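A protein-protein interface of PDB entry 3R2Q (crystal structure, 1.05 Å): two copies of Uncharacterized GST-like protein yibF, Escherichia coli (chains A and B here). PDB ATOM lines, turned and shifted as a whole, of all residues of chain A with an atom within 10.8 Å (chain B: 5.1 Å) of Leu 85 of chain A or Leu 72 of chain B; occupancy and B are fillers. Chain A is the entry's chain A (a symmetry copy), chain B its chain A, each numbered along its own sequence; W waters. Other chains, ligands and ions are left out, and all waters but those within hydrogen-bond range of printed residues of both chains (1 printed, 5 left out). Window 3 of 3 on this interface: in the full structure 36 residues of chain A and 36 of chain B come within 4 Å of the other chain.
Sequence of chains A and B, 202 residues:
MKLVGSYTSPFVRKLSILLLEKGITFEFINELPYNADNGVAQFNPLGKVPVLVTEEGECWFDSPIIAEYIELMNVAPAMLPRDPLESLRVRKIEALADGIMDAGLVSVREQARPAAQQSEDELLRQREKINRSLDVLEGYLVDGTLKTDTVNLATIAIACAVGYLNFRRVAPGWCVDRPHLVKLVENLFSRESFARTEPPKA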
ATOM      1  N   GLU A  68      11.432 -21.375   4.260  1.00  0.00           N
ATOM      2  CA  GLU A  68      10.180 -20.825   4.742  1.00  0.00           C
ATOM      3  C   GLU A  68       9.990 -19.370   4.327  1.00  0.00           C
ATOM      4  O   GLU A  68       8.853 -18.994   4.008  1.00  0.00           O
ATOM      5  CB  GLU A  68      10.021 -20.861   6.252  1.00  0.00           C
ATOM      6  CG  GLU A  68       9.846 -22.290   6.759  1.00  0.00           C
ATOM      7  CD  GLU A  68       9.712 -22.294   8.269  1.00  0.00           C
ATOM      8  OE1 GLU A  68      10.784 -22.474   8.906  1.00  0.00           O
ATOM      9  OE2 GLU A  68       8.618 -22.108   8.804  1.00  0.00           O
ATOM     10  N   LEU A  80       4.959 -25.968   0.283  1.00  0.00           N
ATOM     11  CA  LEU A  80       4.460 -26.385   1.576  1.00  0.00           C
ATOM     12  C   LEU A  80       2.913 -26.310   1.537  1.00  0.00           C
ATOM     13  O   LEU A  80       2.375 -25.389   0.917  1.00  0.00           O
ATOM     14  CB  LEU A  80       4.913 -25.499   2.719  1.00  0.00           C
ATOM     15  CG  LEU A  80       6.407 -25.584   3.029  1.00  0.00           C
ATOM     16  CD1 LEU A  80       6.800 -24.503   4.004  1.00  0.00           C
ATOM     17  CD2 LEU A  80       6.719 -26.964   3.618  1.00  0.00           C
ATOM     18  N   PRO A  81       2.253 -27.226   2.252  1.00  0.00           N
ATOM     19  CA  PRO A  81       0.794 -27.139   2.414  1.00  0.00           C
ATOM     20  C   PRO A  81       0.466 -25.948   3.307  1.00  0.00           C
ATOM     21  O   PRO A  81       1.276 -25.431   4.080  1.00  0.00           O
ATOM     22  CB  PRO A  81       0.422 -28.503   2.965  1.00  0.00           C
ATOM     23  CG  PRO A  81       1.628 -28.952   3.696  1.00  0.00           C
ATOM     24  CD  PRO A  81       2.803 -28.366   2.967  1.00  0.00           C
ATOM     25  N   ARG A  82      -0.787 -25.460   3.241  1.00  0.00           N
ATOM     26  CA  ARG A  82      -1.195 -24.312   4.018  1.00  0.00           C
ATOM     27  C   ARG A  82      -1.471 -24.645   5.469  1.00  0.00           C
ATOM     28  O   ARG A  82      -1.288 -23.817   6.354  1.00  0.00           O
ATOM     29  CB  ARG A  82      -2.472 -23.659   3.451  1.00  0.00           C
ATOM     30  CG  ARG A  82      -2.137 -23.004   2.092  1.00  0.00           C
ATOM     31  CD  ARG A  82      -3.443 -22.572   1.448  1.00  0.00           C
ATOM     32  NE  ARG A  82      -3.239 -22.065   0.112  1.00  0.00           N
ATOM     33  CZ  ARG A  82      -4.211 -21.858  -0.763  1.00  0.00           C
ATOM     34  NH1 ARG A  82      -5.454 -22.137  -0.414  1.00  0.00           N
ATOM     35  NH2 ARG A  82      -3.946 -21.388  -1.972  1.00  0.00           N
ATOM     36  N   ASP A  83      -1.940 -25.848   5.729  1.00  0.00           N
ATOM     37  CA  ASP A  83      -2.285 -26.223   7.079  1.00  0.00           C
ATOM     38  C   ASP A  83      -1.045 -26.241   7.979  1.00  0.00           C
ATOM     39  O   ASP A  83      -0.077 -26.903   7.583  1.00  0.00           O
ATOM     40  CB  ASP A  83      -2.899 -27.626   7.094  1.00  0.00           C
ATOM     41  CG  ASP A  83      -3.183 -28.075   8.507  1.00  0.00           C
ATOM     42  OD1 ASP A  83      -4.108 -27.563   9.166  1.00  0.00           O
ATOM     43  OD2 ASP A  83      -2.489 -29.010   8.990  1.00  0.00           O
ATOM     44  N   PRO A  84      -1.090 -25.575   9.146  1.00  0.00           N
ATOM     45  CA  PRO A  84       0.124 -25.527   9.953  1.00  0.00           C
ATOM     46  C   PRO A  84       0.738 -26.878  10.334  1.00  0.00           C
ATOM     47  O   PRO A  84       1.939 -27.039  10.245  1.00  0.00           O
ATOM     48  CB  PRO A  84      -0.314 -24.739  11.179  1.00  0.00           C
ATOM     49  CG  PRO A  84      -1.385 -23.802  10.589  1.00  0.00           C
ATOM     50  CD  PRO A  84      -2.147 -24.699   9.673  1.00  0.00           C
ATOM     51  N   LEU A  85      -0.087 -27.827  10.778  1.00  0.00           N
ATOM     52  CA  LEU A  85       0.489 -29.096  11.204  1.00  0.00           C
ATOM     53  C   LEU A  85       1.032 -29.869  10.010  1.00  0.00           C
ATOM     54  O   LEU A  85       2.125 -30.455  10.087  1.00  0.00           O
ATOM     55  CB  LEU A  85      -0.542 -29.877  11.992  1.00  0.00           C
ATOM     56  CG  LEU A  85      -0.085 -31.277  12.442  1.00  0.00           C
ATOM     57  CD1 LEU A  85       1.076 -31.158  13.389  1.00  0.00           C
ATOM     58  CD2 LEU A  85      -1.179 -32.066  13.147  1.00  0.00           C
ATOM     59  N   GLU A  86       0.317 -29.907   8.882  1.00  0.00           N
ATOM     60  CA  GLU A  86       0.860 -30.655   7.749  1.00  0.00           C
ATOM     61  C   GLU A  86       2.102 -29.958   7.224  1.00  0.00           C
ATOM     62  O   GLU A  86       3.025 -30.618   6.769  1.00  0.00           O
ATOM     63  CB  GLU A  86      -0.169 -30.888   6.647  1.00  0.00           C
ATOM     64  CG  GLU A  86      -1.267 -31.856   7.051  1.00  0.00           C
ATOM     65  CD  GLU A  86      -0.790 -33.216   7.509  1.00  0.00           C
ATOM     66  OE1 GLU A  86       0.025 -33.841   6.767  1.00  0.00           O
ATOM     67  OE2 GLU A  86      -1.233 -33.593   8.618  1.00  0.00           O
ATOM     68  N   SER A  87       2.178 -28.619   7.255  1.00  0.00           N
ATOM     69  CA  SER A  87       3.401 -27.936   6.863  1.00  0.00           C
ATOM     70  C   SER A  87       4.544 -28.358   7.750  1.00  0.00           C
ATOM     71  O   SER A  87       5.663 -28.637   7.277  1.00  0.00           O
ATOM     72  CB  SER A  87       3.159 -26.431   6.899  1.00  0.00           C
ATOM     73  OG  SER A  87       4.443 -25.805   6.640  1.00  0.00           O
ATOM     74  N   LEU A  88       4.320 -28.400   9.059  1.00  0.00           N
ATOM     75  CA  LEU A  88       5.353 -28.838   9.976  1.00  0.00           C
ATOM     76  C   LEU A  88       5.765 -30.268   9.709  1.00  0.00           C
ATOM     77  O   LEU A  88       6.972 -30.575   9.816  1.00  0.00           O
ATOM     78  CB  LEU A  88       4.900 -28.627  11.416  1.00  0.00           C
ATOM     79  CG  LEU A  88       6.029 -28.616  12.422  1.00  0.00           C
ATOM     80  CD1 LEU A  88       7.017 -27.514  12.282  1.00  0.00           C
ATOM     81  CD2 LEU A  88       5.440 -28.561  13.842  1.00  0.00           C
ATOM     82  N   ARG A  89       4.861 -31.159   9.368  1.00  0.00           N
ATOM     83  CA  ARG A  89       5.228 -32.525   9.044  1.00  0.00           C
ATOM     84  C   ARG A  89       6.120 -32.572   7.820  1.00  0.00           C
ATOM     85  O   ARG A  89       7.098 -33.302   7.786  1.00  0.00           O
ATOM     86  CB  ARG A  89       3.963 -33.382   8.828  1.00  0.00           C
ATOM     87  CG  ARG A  89       3.254 -33.760  10.108  1.00  0.00           C
ATOM     88  CD  ARG A  89       2.096 -34.751   9.920  1.00  0.00           C
ATOM     89  NE  ARG A  89       1.642 -35.226  11.205  1.00  0.00           N
ATOM     90  CZ  ARG A  89       0.476 -35.307  11.711  1.00  0.00           C
ATOM     91  NH1 ARG A  89      -0.631 -34.879  11.032  1.00  0.00           N
ATOM     92  NH2 ARG A  89       0.229 -35.778  12.934  1.00  0.00           N
ATOM     93  N   VAL A  90       5.809 -31.788   6.776  1.00  0.00           N
ATOM     94  CA  VAL A  90       6.727 -31.699   5.614  1.00  0.00           C
ATOM     95  C   VAL A  90       8.070 -31.233   6.049  1.00  0.00           C
ATOM     96  O   VAL A  90       9.108 -31.764   5.585  1.00  0.00           O
ATOM     97  CB  VAL A  90       6.119 -30.793   4.530  1.00  0.00           C
ATOM     98  CG1 VAL A  90       7.104 -30.644   3.383  1.00  0.00           C
ATOM     99  CG2 VAL A  90       4.833 -31.381   3.987  1.00  0.00           C
ATOM    100  N   ARG A  91       8.137 -30.213   6.904  1.00  0.00           N
ATOM    101  CA  ARG A  91       9.390 -29.674   7.404  1.00  0.00           C
ATOM    102  C   ARG A  91      10.152 -30.631   8.326  1.00  0.00           C
ATOM    103  O   ARG A  91      11.389 -30.596   8.371  1.00  0.00           O
ATOM    104  CB  ARG A  91       9.194 -28.268   8.025  1.00  0.00           C
ATOM    105  CG  ARG A  91       8.993 -27.232   6.920  1.00  0.00           C
ATOM    106  CD  ARG A  91       8.678 -25.858   7.470  1.00  0.00           C
ATOM    107  NE  ARG A  91       7.289 -25.831   7.890  1.00  0.00           N
ATOM    108  CZ  ARG A  91       6.783 -25.035   8.839  1.00  0.00           C
ATOM    109  NH1 ARG A  91       7.482 -24.208   9.594  1.00  0.00           N
ATOM    110  NH2 ARG A  91       5.455 -25.130   9.035  1.00  0.00           N
ATOM    111  N   LYS A  92       9.487 -31.557   8.998  1.00  0.00           N
ATOM    112  CA  LYS A  92      10.162 -32.629   9.724  1.00  0.00           C
ATOM    113  C   LYS A  92      10.896 -33.515   8.744  1.00  0.00           C
ATOM    114  O   LYS A  92      12.050 -33.894   8.943  1.00  0.00           O
ATOM    115  CB  LYS A  92       9.137 -33.391  10.575  1.00  0.00           C
ATOM    116  CG  LYS A  92       9.627 -34.197  11.678  1.00  0.00           C
ATOM    117  CD  LYS A  92      10.502 -35.346  11.501  1.00  0.00           C
ATOM    118  CE  LYS A  92       9.773 -36.530  10.869  1.00  0.00           C
ATOM    119  NZ  LYS A  92       8.621 -37.043  11.580  1.00  0.00           N
ATOM    120  N   ILE A  93      10.247 -33.856   7.622  1.00  0.00           N
ATOM    121  CA  ILE A  93      10.901 -34.668   6.600  1.00  0.00           C
ATOM    122  C   ILE A  93      12.055 -33.896   5.971  1.00  0.00           C
ATOM    123  O   ILE A  93      13.108 -34.459   5.691  1.00  0.00           O
ATOM    124  CB  ILE A  93       9.896 -35.233   5.598  1.00  0.00           C
ATOM    125  CG1 ILE A  93       8.816 -36.047   6.297  1.00  0.00           C
ATOM    126  CG2 ILE A  93      10.606 -36.056   4.527  1.00  0.00           C
ATOM    127  CD1 ILE A  93       7.743 -36.588   5.354  1.00  0.00           C
ATOM    128  N   THR A 145       3.025 -41.916   3.192  1.00  0.00           N
ATOM    129  CA  THR A 145       3.394 -40.648   3.828  1.00  0.00           C
ATOM    130  C   THR A 145       4.019 -39.700   2.833  1.00  0.00           C
ATOM    131  O   THR A 145       3.792 -38.486   2.865  1.00  0.00           O
ATOM    132  CB  THR A 145       4.404 -40.921   4.992  1.00  0.00           C
ATOM    133  OG1 THR A 145       3.792 -41.791   5.920  1.00  0.00           O
ATOM    134  CG2 THR A 145       4.774 -39.592   5.667  1.00  0.00           C
ATOM    135  N   ASN A 152       7.569 -31.326  -3.208  1.00  0.00           N
ATOM    136  CA  ASN A 152       7.402 -30.337  -2.152  1.00  0.00           C
ATOM    137  C   ASN A 152       8.765 -30.085  -1.532  1.00  0.00           C
ATOM    138  O   ASN A 152       9.770 -30.627  -1.975  1.00  0.00           O
ATOM    139  CB  ASN A 152       6.302 -30.736  -1.163  1.00  0.00           C
ATOM    140  CG  ASN A 152       6.645 -31.925  -0.317  1.00  0.00           C
ATOM    141  OD1 ASN A 152       7.806 -32.319  -0.194  1.00  0.00           O
ATOM    142  ND2 ASN A 152       5.620 -32.472   0.333  1.00  0.00           N
ATOM    143  N   TRP B  60       9.142 -36.407  16.456  1.00  0.00           N
ATOM    144  CA  TRP B  60       9.468 -35.088  15.911  1.00  0.00           C
ATOM    145  C   TRP B  60      10.915 -34.757  16.185  1.00  0.00           C
ATOM    146  O   TRP B  60      11.405 -34.945  17.312  1.00  0.00           O
ATOM    147  CB  TRP B  60       8.573 -34.017  16.522  1.00  0.00           C
ATOM    148  CG  TRP B  60       7.136 -34.182  16.140  1.00  0.00           C
ATOM    149  CD1 TRP B  60       6.164 -34.927  16.767  1.00  0.00           C
ATOM    150  CD2 TRP B  60       6.500 -33.577  15.013  1.00  0.00           C
ATOM    151  NE1 TRP B  60       4.983 -34.794  16.062  1.00  0.00           N
ATOM    152  CE2 TRP B  60       5.187 -33.975  15.010  1.00  0.00           C
ATOM    153  CE3 TRP B  60       6.940 -32.723  14.007  1.00  0.00           C
ATOM    154  CZ2 TRP B  60       4.263 -33.540  14.018  1.00  0.00           C
ATOM    155  CZ3 TRP B  60       6.034 -32.308  13.039  1.00  0.00           C
ATOM    156  CH2 TRP B  60       4.750 -32.702  13.053  1.00  0.00           C
ATOM    157  N   GLU B  68       8.537 -25.528  17.300  1.00  0.00           N
ATOM    158  CA  GLU B  68       7.350 -25.095  16.590  1.00  0.00           C
ATOM    159  C   GLU B  68       6.147 -25.989  16.875  1.00  0.00           C
ATOM    160  O   GLU B  68       5.033 -25.457  16.983  1.00  0.00           O
ATOM    161  CB  GLU B  68       7.503 -25.057  15.080  1.00  0.00           C
ATOM    162  CG  GLU B  68       8.444 -23.936  14.644  1.00  0.00           C
ATOM    163  CD  GLU B  68       8.594 -23.939  13.135  1.00  0.00           C
ATOM    164  OE1 GLU B  68       9.577 -24.588  12.691  1.00  0.00           O
ATOM    165  OE2 GLU B  68       7.776 -23.355  12.422  1.00  0.00           O
ATOM    166  N   TYR B  69       6.366 -27.302  16.945  1.00  0.00           N
ATOM    167  CA  TYR B  69       5.260 -28.207  17.294  1.00  0.00           C
ATOM    168  C   TYR B  69       4.653 -27.787  18.610  1.00  0.00           C
ATOM    169  O   TYR B  69       3.444 -27.707  18.767  1.00  0.00           O
ATOM    170  CB  TYR B  69       5.770 -29.670  17.312  1.00  0.00           C
ATOM    171  CG  TYR B  69       4.684 -30.613  17.735  1.00  0.00           C
ATOM    172  CD1 TYR B  69       3.853 -31.176  16.766  1.00  0.00           C
ATOM    173  CD2 TYR B  69       4.490 -30.987  19.027  1.00  0.00           C
ATOM    174  CE1 TYR B  69       2.847 -32.087  17.111  1.00  0.00           C
ATOM    175  CE2 TYR B  69       3.474 -31.839  19.402  1.00  0.00           C
ATOM    176  CZ  TYR B  69       2.654 -32.385  18.432  1.00  0.00           C
ATOM    177  OH  TYR B  69       1.640 -33.251  18.786  1.00  0.00           O
ATOM    178  N   ILE B  70       5.510 -27.573  19.616  1.00  0.00           N
ATOM    179  CA  ILE B  70       5.035 -27.160  20.945  1.00  0.00           C
ATOM    180  C   ILE B  70       4.265 -25.855  20.821  1.00  0.00           C
ATOM    181  O   ILE B  70       3.203 -25.698  21.422  1.00  0.00           O
ATOM    182  CB  ILE B  70       6.189 -27.108  21.936  1.00  0.00           C
ATOM    183  CG1 ILE B  70       6.792 -28.530  22.149  1.00  0.00           C
ATOM    184  CG2 ILE B  70       5.815 -26.454  23.250  1.00  0.00           C
ATOM    185  CD1 ILE B  70       8.150 -28.478  22.791  1.00  0.00           C
ATOM    186  N   GLU B  71       4.800 -24.903  20.062  1.00  0.00           N
ATOM    187  CA  GLU B  71       4.134 -23.606  19.896  1.00  0.00           C
ATOM    188  C   GLU B  71       2.761 -23.761  19.291  1.00  0.00           C
ATOM    189  O   GLU B  71       1.870 -23.003  19.654  1.00  0.00           O
ATOM    190  CB  GLU B  71       4.979 -22.644  19.048  1.00  0.00           C
ATOM    191  CG  GLU B  71       5.799 -21.728  19.897  1.00  0.00           C
ATOM    192  CD  GLU B  71       5.192 -20.907  21.006  1.00  0.00           C
ATOM    193  OE1 GLU B  71       4.387 -19.980  20.701  1.00  0.00           O
ATOM    194  OE2 GLU B  71       5.516 -21.084  22.206  1.00  0.00           O
ATOM    195  N   LEU B  72       2.588 -24.679  18.386  1.00  0.00           N
ATOM    196  CA  LEU B  72       1.330 -24.943  17.710  1.00  0.00           C
ATOM    197  C   LEU B  72       0.292 -25.441  18.699  1.00  0.00           C
ATOM    198  O   LEU B  72      -0.886 -25.224  18.451  1.00  0.00           O
ATOM    199  CB  LEU B  72       1.609 -25.898  16.525  1.00  0.00           C
ATOM    200  CG  LEU B  72       0.422 -26.066  15.558  1.00  0.00           C
ATOM    201  CD1 LEU B  72      -0.042 -24.737  15.000  1.00  0.00           C
ATOM    202  CD2 LEU B  72       0.759 -27.013  14.411  1.00  0.00           C
ATOM    203  N   MET B  73       0.752 -26.072  19.782  1.00  0.00           N
ATOM    204  CA  MET B  73      -0.210 -26.522  20.790  1.00  0.00           C
ATOM    205  C   MET B  73      -0.888 -25.231  21.241  1.00  0.00           C
ATOM    206  O   MET B  73      -1.980 -25.561  21.710  1.00  0.00           O
ATOM    207  CB  MET B  73       0.396 -27.263  21.956  1.00  0.00           C
ATOM    208  CG  MET B  73       1.201 -28.438  21.417  1.00  0.00           C
ATOM    209  SD  MET B  73       2.194 -29.208  22.689  1.00  0.00           S
ATOM    210  CE  MET B  73       0.943 -29.687  23.890  1.00  0.00           C
ATOM    211  N   ASN B  74      -0.560 -23.962  21.243  1.00  0.00           N
ATOM    212  CA  ASN B  74      -1.302 -22.805  21.670  1.00  0.00           C
ATOM    213  C   ASN B  74      -1.511 -22.784  23.154  1.00  0.00           C
ATOM    214  O   ASN B  74      -2.556 -22.418  23.604  1.00  0.00           O
ATOM    215  CB  ASN B  74      -2.485 -22.630  20.774  1.00  0.00           C
ATOM    216  CG  ASN B  74      -3.121 -21.273  20.766  1.00  0.00           C
ATOM    217  OD1 ASN B  74      -2.356 -20.312  20.826  1.00  0.00           O
ATOM    218  ND2 ASN B  74      -4.380 -21.343  20.438  1.00  0.00           N
HETATM  219  O   HOH W   1       5.700 -21.725  10.379  1.00  0.00           O
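OE2 of Glu 68 of chain A touches OE2 of Glu 68 of chain B (3.9 Å).
CD1 of Leu 72 of chain B touches CB of Pro 84 of chain A (3.8 Å).
Trp 60 of chain B touches Leu 85 of chain A.
Leu 85 of chain A touches Leu 72 of chain B.
CG of Leu 88 of chain A touches CZ3 of Trp 60 of chain B (3.7 Å).
CB of Glu 68 of chain B touches CD1 of Leu 88 of chain A (3.8 Å).
Tyr 69 of chain B touches Leu 88 of chain A (N to CD2, 3.5 Å).
CG of Arg 89 of chain A touches CH2 of Trp 60 of chain B, 3.5 Å away.
Trp 60 of chain B touches Lys 92 of chain A.
Glu 68 of chain A touches its own counterpart, Glu 68 of chain B.
Position printed for both chains: 68.
Of the 10 pairs that touch across the chains among the printed residues, 1 has its exchanged pair printed and touching as well.
The side-chain carboxylate (OE2) of Glu 68 of chain B lies within salt-bridge range of the guanidinium group (NH1) of Arg 91 of chain A.
Water W1 lies within hydrogen-bond range of the guanidinium group of Arg 91 of chain A (3.2 Å), the side-chain carboxylate of Glu 68 of chain A (3.3 Å) and the side-chain carboxylate of Glu 68 of chain B (3.3 Å).
Hydrophobic or aromatic side chains of chain A within 4 Å of the printed part of chain B: Pro 84, Leu 85 and Leu 88.
Among the printed residues, 10 pairs touch across the chains.
Among the printed residues, Asp or Glu carboxylates within 4 Å of a Lys or Arg side-chain nitrogen of the other chain: Arg 91 of chain A with Glu 68 of chain B.
Printed residues of chain B within 4 Å of Pro 84 of chain A: Leu 72.
Of the printed residues of chain B, Leu 85 of chain A touches Trp 60 and Leu 72.
Of the printed residues of chain B, Leu 88 of chain A touches Trp 60 (3.7 Å), Glu 68 (3.8 Å) and Tyr 69 (3.5 Å).
Printed residues of chain B within 4 Å of Arg 89 of chain A: Trp 60.
Of the printed residues of chain A, Trp 60 of chain B touches Leu 85 (3.999 Å), Leu 88 (3.7 Å), Arg 89 (3.5 Å) and Lys 92 (3.8 Å).
Of the printed residues of chain A, Glu 68 of chain B touches Glu 68, Leu 88 and Arg 91.
Of the printed residues of chain A, Leu 72 of chain B touches Pro 84 (3.8 Å) and Leu 85 (3.8 Å).
Asn 74 of chain B touches none of the printed residues of chain A.
The nearest printed residue of chain A that does not touch Leu 72 of chain B is Leu 88 of chain A (5.0 Å).
N of Leu 85 of chain A is in hydrogen-bond range of OD2 of Asp 83 of chain A.
The guanidinium group (NH1) of Arg 91 of chain A lies within salt-bridge range of the side-chain carboxylate (OE2) of Glu 68 of chain A.
The guanidinium group of Arg 89 of chain A is in salt-bridge range of the side-chain carboxylate of Glu 86 of chain A (2.8 Å).
OG of Ser 87 of chain A sits at hydrogen-bond distance from NH2 of Arg 91 of chain A, at 2.7 Å.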
